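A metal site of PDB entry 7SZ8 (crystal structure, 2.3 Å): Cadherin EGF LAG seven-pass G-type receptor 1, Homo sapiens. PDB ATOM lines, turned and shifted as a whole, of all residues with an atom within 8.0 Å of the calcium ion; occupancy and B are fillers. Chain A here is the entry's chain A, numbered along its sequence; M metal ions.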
ATOM      1  N   VAL A   3     -26.743  13.936  19.461  1.00  0.00           N
ATOM      2  CA  VAL A   3     -27.546  14.898  20.288  1.00  0.00           C
ATOM      3  C   VAL A   3     -28.168  14.126  21.465  1.00  0.00           C
ATOM      4  O   VAL A   3     -28.984  13.207  21.215  1.00  0.00           O
ATOM      5  CB  VAL A   3     -28.629  15.617  19.452  1.00  0.00           C
ATOM      6  CG1 VAL A   3     -29.441  16.589  20.308  1.00  0.00           C
ATOM      7  CG2 VAL A   3     -28.032  16.328  18.240  1.00  0.00           C
ATOM      8  N   ASN A   4     -27.824  14.512  22.695  1.00  0.00           N
ATOM      9  CA  ASN A   4     -28.162  13.816  23.971  1.00  0.00           C
ATOM     10  C   ASN A   4     -29.491  14.357  24.536  1.00  0.00           C
ATOM     11  O   ASN A   4     -29.447  15.327  25.300  1.00  0.00           O
ATOM     12  CB  ASN A   4     -27.017  13.994  24.975  1.00  0.00           C
ATOM     13  CG  ASN A   4     -27.106  13.051  26.168  1.00  0.00           C
ATOM     14  OD1 ASN A   4     -27.745  12.006  26.072  1.00  0.00           O
ATOM     15  ND2 ASN A   4     -26.501  13.428  27.283  1.00  0.00           N
ATOM     16  N   ASP A   5     -30.626  13.706  24.223  1.00  0.00           N
ATOM     17  CA  ASP A   5     -32.000  14.239  24.485  1.00  0.00           C
ATOM     18  C   ASP A   5     -32.682  13.555  25.689  1.00  0.00           C
ATOM     19  O   ASP A   5     -33.745  14.068  26.092  1.00  0.00           O
ATOM     20  CB  ASP A   5     -32.922  14.056  23.272  1.00  0.00           C
ATOM     21  CG  ASP A   5     -32.688  15.042  22.143  1.00  0.00           C
ATOM     22  OD1 ASP A   5     -32.274  16.189  22.428  1.00  0.00           O
ATOM     23  OD2 ASP A   5     -32.916  14.658  20.990  1.00  0.00           O
ATOM     24  N   ASN A   6     -32.138  12.469  26.238  1.00  0.00           N
ATOM     25  CA  ASN A   6     -32.871  11.660  27.261  1.00  0.00           C
ATOM     26  C   ASN A   6     -32.086  11.560  28.574  1.00  0.00           C
ATOM     27  O   ASN A   6     -30.895  11.148  28.541  1.00  0.00           O
ATOM     28  CB  ASN A   6     -33.219  10.270  26.732  1.00  0.00           C
ATOM     29  CG  ASN A   6     -34.129  10.343  25.515  1.00  0.00           C
ATOM     30  OD1 ASN A   6     -35.196  10.957  25.566  1.00  0.00           O
ATOM     31  ND2 ASN A   6     -33.726   9.707  24.423  1.00  0.00           N
ATOM     32  N   GLU A   7     -32.754  11.911  29.679  1.00  0.00           N
ATOM     33  CA  GLU A   7     -32.299  11.718  31.082  1.00  0.00           C
ATOM     34  C   GLU A   7     -32.424  10.228  31.410  1.00  0.00           C
ATOM     35  O   GLU A   7     -33.430   9.616  31.050  1.00  0.00           O
ATOM     36  CB  GLU A   7     -33.130  12.572  32.048  1.00  0.00           C
ATOM     37  CG  GLU A   7     -32.436  12.857  33.379  1.00  0.00           C
ATOM     38  CD  GLU A   7     -33.179  13.859  34.256  1.00  0.00           C
ATOM     39  OE1 GLU A   7     -32.753  15.028  34.328  1.00  0.00           O
ATOM     40  OE2 GLU A   7     -34.172  13.458  34.892  1.00  0.00           O
ATOM     41  N   PRO A   8     -31.427   9.599  32.092  1.00  0.00           N
ATOM     42  CA  PRO A   8     -31.562   8.224  32.570  1.00  0.00           C
ATOM     43  C   PRO A   8     -32.714   8.134  33.569  1.00  0.00           C
ATOM     44  O   PRO A   8     -32.742   8.913  34.498  1.00  0.00           O
ATOM     45  CB  PRO A   8     -30.244   7.884  33.272  1.00  0.00           C
ATOM     46  CG  PRO A   8     -29.295   8.997  32.876  1.00  0.00           C
ATOM     47  CD  PRO A   8     -30.139  10.187  32.471  1.00  0.00           C
ATOM     48  N   VAL A  35     -32.455   3.222  32.430  1.00  0.00           N
ATOM     49  CA  VAL A  35     -32.626   3.078  30.965  1.00  0.00           C
ATOM     50  C   VAL A  35     -32.486   4.486  30.384  1.00  0.00           C
ATOM     51  O   VAL A  35     -33.343   5.339  30.675  1.00  0.00           O
ATOM     52  CB  VAL A  35     -33.963   2.425  30.579  1.00  0.00           C
ATOM     53  CG1 VAL A  35     -34.103   2.249  29.069  1.00  0.00           C
ATOM     54  CG2 VAL A  35     -34.161   1.094  31.291  1.00  0.00           C
ATOM     55  N   ASP A  36     -31.401   4.724  29.668  1.00  0.00           N
ATOM     56  CA  ASP A  36     -31.231   5.954  28.864  1.00  0.00           C
ATOM     57  C   ASP A  36     -31.976   5.693  27.559  1.00  0.00           C
ATOM     58  O   ASP A  36     -31.841   4.559  27.062  1.00  0.00           O
ATOM     59  CB  ASP A  36     -29.746   6.242  28.700  1.00  0.00           C
ATOM     60  CG  ASP A  36     -29.472   7.652  28.267  1.00  0.00           C
ATOM     61  OD1 ASP A  36     -29.722   7.961  27.085  1.00  0.00           O
ATOM     62  OD2 ASP A  36     -29.028   8.442  29.121  1.00  0.00           O
ATOM     63  N   ALA A  37     -32.763   6.655  27.068  1.00  0.00           N
ATOM     64  CA  ALA A  37     -33.665   6.455  25.899  1.00  0.00           C
ATOM     65  C   ALA A  37     -32.914   6.701  24.569  1.00  0.00           C
ATOM     66  O   ALA A  37     -33.495   6.401  23.509  1.00  0.00           O
ATOM     67  CB  ALA A  37     -34.909   7.304  26.037  1.00  0.00           C
ATOM     68  N   ASP A  38     -31.669   7.205  24.602  1.00  0.00           N
ATOM     69  CA  ASP A  38     -30.811   7.393  23.395  1.00  0.00           C
ATOM     70  C   ASP A  38     -30.107   6.071  23.040  1.00  0.00           C
ATOM     71  O   ASP A  38     -30.498   4.992  23.585  1.00  0.00           O
ATOM     72  CB  ASP A  38     -29.755   8.483  23.622  1.00  0.00           C
ATOM     73  CG  ASP A  38     -30.345   9.796  24.094  1.00  0.00           C
ATOM     74  OD1 ASP A  38     -31.264  10.292  23.430  1.00  0.00           O
ATOM     75  OD2 ASP A  38     -29.893  10.292  25.139  1.00  0.00           O
ATOM     76  N   SER A  39     -29.116   6.157  22.153  1.00  0.00           N
ATOM     77  CA  SER A  39     -28.103   5.095  21.891  1.00  0.00           C
ATOM     78  C   SER A  39     -26.685   5.684  21.976  1.00  0.00           C
ATOM     79  O   SER A  39     -26.540   6.899  22.258  1.00  0.00           O
ATOM     80  CB  SER A  39     -28.373   4.451  20.549  1.00  0.00           C
ATOM     81  OG  SER A  39     -28.487   5.447  19.551  1.00  0.00           O
ATOM     82  N   GLY A  40     -25.670   4.833  21.764  1.00  0.00           N
ATOM     83  CA  GLY A  40     -24.244   5.215  21.768  1.00  0.00           C
ATOM     84  C   GLY A  40     -23.754   5.534  23.174  1.00  0.00           C
ATOM     85  O   GLY A  40     -24.122   4.784  24.112  1.00  0.00           O
ATOM     86  N   GLU A  41     -22.946   6.582  23.290  1.00  0.00           N
ATOM     87  CA  GLU A  41     -22.402   7.110  24.578  1.00  0.00           C
ATOM     88  C   GLU A  41     -23.456   8.030  25.214  1.00  0.00           C
ATOM     89  O   GLU A  41     -23.400   8.249  26.443  1.00  0.00           O
ATOM     90  CB  GLU A  41     -21.052   7.793  24.328  1.00  0.00           C
ATOM     91  CG  GLU A  41     -20.022   6.921  23.606  1.00  0.00           C
ATOM     92  CD  GLU A  41     -19.363   5.789  24.397  1.00  0.00           C
ATOM     93  OE1 GLU A  41     -19.270   5.902  25.619  1.00  0.00           O
ATOM     94  OE2 GLU A  41     -18.947   4.794  23.773  1.00  0.00           O
ATOM     95  N   ASN A  42     -24.396   8.555  24.414  1.00  0.00           N
ATOM     96  CA  ASN A  42     -25.581   9.318  24.907  1.00  0.00           C
ATOM     97  C   ASN A  42     -26.381   8.431  25.863  1.00  0.00           C
ATOM     98  O   ASN A  42     -27.250   8.976  26.575  1.00  0.00           O
ATOM     99  CB  ASN A  42     -26.545   9.741  23.794  1.00  0.00           C
ATOM    100  CG  ASN A  42     -26.011  10.805  22.856  1.00  0.00           C
ATOM    101  OD1 ASN A  42     -26.162  10.693  21.641  1.00  0.00           O
ATOM    102  ND2 ASN A  42     -25.440  11.864  23.390  1.00  0.00           N
ATOM    103  N   ALA A  43     -26.154   7.112  25.802  1.00  0.00           N
ATOM    104  CA  ALA A  43     -26.999   6.105  26.475  1.00  0.00           C
ATOM    105  C   ALA A  43     -26.203   5.310  27.504  1.00  0.00           C
ATOM    106  O   ALA A  43     -26.844   4.685  28.363  1.00  0.00           O
ATOM    107  CB  ALA A  43     -27.617   5.171  25.474  1.00  0.00           C
ATOM    108  N   ARG A  44     -24.877   5.280  27.371  1.00  0.00           N
ATOM    109  CA  ARG A  44     -23.940   4.550  28.260  1.00  0.00           C
ATOM    110  C   ARG A  44     -23.991   5.190  29.655  1.00  0.00           C
ATOM    111  O   ARG A  44     -23.843   6.436  29.744  1.00  0.00           O
ATOM    112  CB  ARG A  44     -22.539   4.581  27.653  1.00  0.00           C
ATOM    113  CG  ARG A  44     -21.528   3.732  28.407  1.00  0.00           C
ATOM    114  CD  ARG A  44     -20.470   3.174  27.475  1.00  0.00           C
ATOM    115  NE  ARG A  44     -19.152   3.251  28.077  1.00  0.00           N
ATOM    116  CZ  ARG A  44     -18.045   2.732  27.546  1.00  0.00           C
ATOM    117  NH1 ARG A  44     -18.092   2.086  26.389  1.00  0.00           N
ATOM    118  NH2 ARG A  44     -16.886   2.868  28.183  1.00  0.00           N
ATOM    119  N   LEU A  45     -24.214   4.371  30.677  1.00  0.00           N
ATOM    120  CA  LEU A  45     -24.503   4.824  32.066  1.00  0.00           C
ATOM    121  C   LEU A  45     -23.366   4.390  32.988  1.00  0.00           C
ATOM    122  O   LEU A  45     -22.868   3.251  32.845  1.00  0.00           O
ATOM    123  CB  LEU A  45     -25.852   4.245  32.518  1.00  0.00           C
ATOM    124  CG  LEU A  45     -27.087   4.797  31.800  1.00  0.00           C
ATOM    125  CD1 LEU A  45     -28.370   4.460  32.534  1.00  0.00           C
ATOM    126  CD2 LEU A  45     -26.999   6.301  31.619  1.00  0.00           C
ATOM    127  N   VAL A 105     -25.513   8.529  35.402  1.00  0.00           N
ATOM    128  CA  VAL A 105     -24.922   9.611  34.567  1.00  0.00           C
ATOM    129  C   VAL A 105     -24.590   8.978  33.218  1.00  0.00           C
ATOM    130  O   VAL A 105     -24.016   7.870  33.248  1.00  0.00           O
ATOM    131  CB  VAL A 105     -23.666  10.187  35.267  1.00  0.00           C
ATOM    132  CG1 VAL A 105     -22.575  10.577  34.295  1.00  0.00           C
ATOM    133  CG2 VAL A 105     -24.008  11.359  36.170  1.00  0.00           C
ATOM    134  N   ASP A 106     -24.961   9.634  32.107  1.00  0.00           N
ATOM    135  CA  ASP A 106     -24.602   9.211  30.729  1.00  0.00           C
ATOM    136  C   ASP A 106     -23.308   9.915  30.333  1.00  0.00           C
ATOM    137  O   ASP A 106     -23.068  11.017  30.833  1.00  0.00           O
ATOM    138  CB  ASP A 106     -25.731   9.450  29.705  1.00  0.00           C
ATOM    139  CG  ASP A 106     -26.321  10.849  29.526  1.00  0.00           C
ATOM    140  OD1 ASP A 106     -25.716  11.844  29.988  1.00  0.00           O
ATOM    141  OD2 ASP A 106     -27.385  10.941  28.893  1.00  0.00           O
ATOM    142  N   HIS A 107     -22.500   9.284  29.474  1.00  0.00           N
ATOM    143  CA  HIS A 107     -21.294   9.926  28.887  1.00  0.00           C
ATOM    144  C   HIS A 107     -21.716  10.840  27.728  1.00  0.00           C
ATOM    145  O   HIS A 107     -21.343  10.511  26.583  1.00  0.00           O
ATOM    146  CB  HIS A 107     -20.263   8.870  28.455  1.00  0.00           C
ATOM    147  CG  HIS A 107     -18.891   9.420  28.228  1.00  0.00           C
ATOM    148  ND1 HIS A 107     -17.948   8.731  27.494  1.00  0.00           N
ATOM    149  CD2 HIS A 107     -18.312  10.578  28.612  1.00  0.00           C
ATOM    150  CE1 HIS A 107     -16.836   9.447  27.448  1.00  0.00           C
ATOM    151  NE2 HIS A 107     -17.025  10.584  28.132  1.00  0.00           N
ATOM    152  N   GLY A 108     -22.483  11.898  28.004  1.00  0.00           N
ATOM    153  CA  GLY A 108     -22.963  12.860  26.987  1.00  0.00           C
ATOM    154  C   GLY A 108     -22.216  14.179  27.114  1.00  0.00           C
ATOM    155  O   GLY A 108     -21.889  14.521  28.267  1.00  0.00           O
ATOM    156  N   PRO A 110     -22.945  17.455  26.674  1.00  0.00           N
ATOM    157  CA  PRO A 110     -23.738  17.887  27.824  1.00  0.00           C
ATOM    158  C   PRO A 110     -24.297  16.627  28.498  1.00  0.00           C
ATOM    159  O   PRO A 110     -25.223  16.016  27.991  1.00  0.00           O
ATOM    160  CB  PRO A 110     -24.819  18.753  27.175  1.00  0.00           C
ATOM    161  CG  PRO A 110     -25.037  18.112  25.796  1.00  0.00           C
ATOM    162  CD  PRO A 110     -23.761  17.378  25.447  1.00  0.00           C
ATOM    163  N   PRO A 111     -23.708  16.137  29.616  1.00  0.00           N
ATOM    164  CA  PRO A 111     -24.179  14.901  30.242  1.00  0.00           C
ATOM    165  C   PRO A 111     -25.388  15.129  31.157  1.00  0.00           C
ATOM    166  O   PRO A 111     -25.364  16.089  31.891  1.00  0.00           O
ATOM    167  CB  PRO A 111     -22.973  14.437  31.071  1.00  0.00           C
ATOM    168  CG  PRO A 111     -22.283  15.738  31.457  1.00  0.00           C
ATOM    169  CD  PRO A 111     -22.588  16.736  30.346  1.00  0.00           C
ATOM    170  N   MET A 112     -26.379  14.250  31.115  1.00  0.00           N
ATOM    171  CA  MET A 112     -27.558  14.295  32.040  1.00  0.00           C
ATOM    172  C   MET A 112     -27.490  13.119  33.023  1.00  0.00           C
ATOM    173  O   MET A 112     -26.864  12.087  32.726  1.00  0.00           O
ATOM    174  CB  MET A 112     -28.867  14.244  31.265  1.00  0.00           C
ATOM    175  CG  MET A 112     -29.114  15.489  30.436  1.00  0.00           C
ATOM    176  SD  MET A 112     -30.333  15.273  29.119  1.00  0.00           S
ATOM    177  CE  MET A 112     -29.514  14.077  28.074  1.00  0.00           C
ATOM    178  N   SER A 113     -28.152  13.310  34.164  1.00  0.00           N
ATOM    179  CA  SER A 113     -28.167  12.377  35.310  1.00  0.00           C
ATOM    180  C   SER A 113     -29.531  12.440  36.001  1.00  0.00           C
ATOM    181  O   SER A 113     -30.219  13.502  35.879  1.00  0.00           O
ATOM    182  CB  SER A 113     -27.079  12.736  36.274  1.00  0.00           C
ATOM    183  OG  SER A 113     -27.427  13.893  37.027  1.00  0.00           O
HETATM  184 CA    CA M   1     -28.899  10.179  27.401  1.00  0.00          CA
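The calcium ion is bound by O of Asn 42, 2.2 Å away.
The calcium ion is bound by OD2 of Asp 106 (2.3 Å).
The calcium ion is bound by the side-chain carboxylate (OD1) of Asp 36 (2.4 Å).
OD2 of Asp 36 is bound to the calcium ion.
The calcium ion is bound by the side-chain carboxylate (OD2) of Asp 38 (2.5 Å).
The backbone carbonyl oxygen (O) of Asn 6 is bound to the calcium ion, at 2.5 Å.
OD1 of Asn 4 is bound to the calcium ion (2.5 Å).
O of Ala 37 lies close to ND2 of Asn 6.
O of Pro 110 is in hydrogen-bond range of ND2 of Asn 4 (3.0 Å).
The side-chain carboxylate (OD1) of Asp 106 sits at hydrogen-bond distance from the backbone NH (N) of Met 112, 2.7 Å away.
Six residues have an atom within 4 Å of the calcium ion: Asn 4, Asn 6, Asp 36, Asp 38, Asn 42 and Asp 106.
The nearest printed residue that does not touch the calcium ion is Met 112 (4.003 Å).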
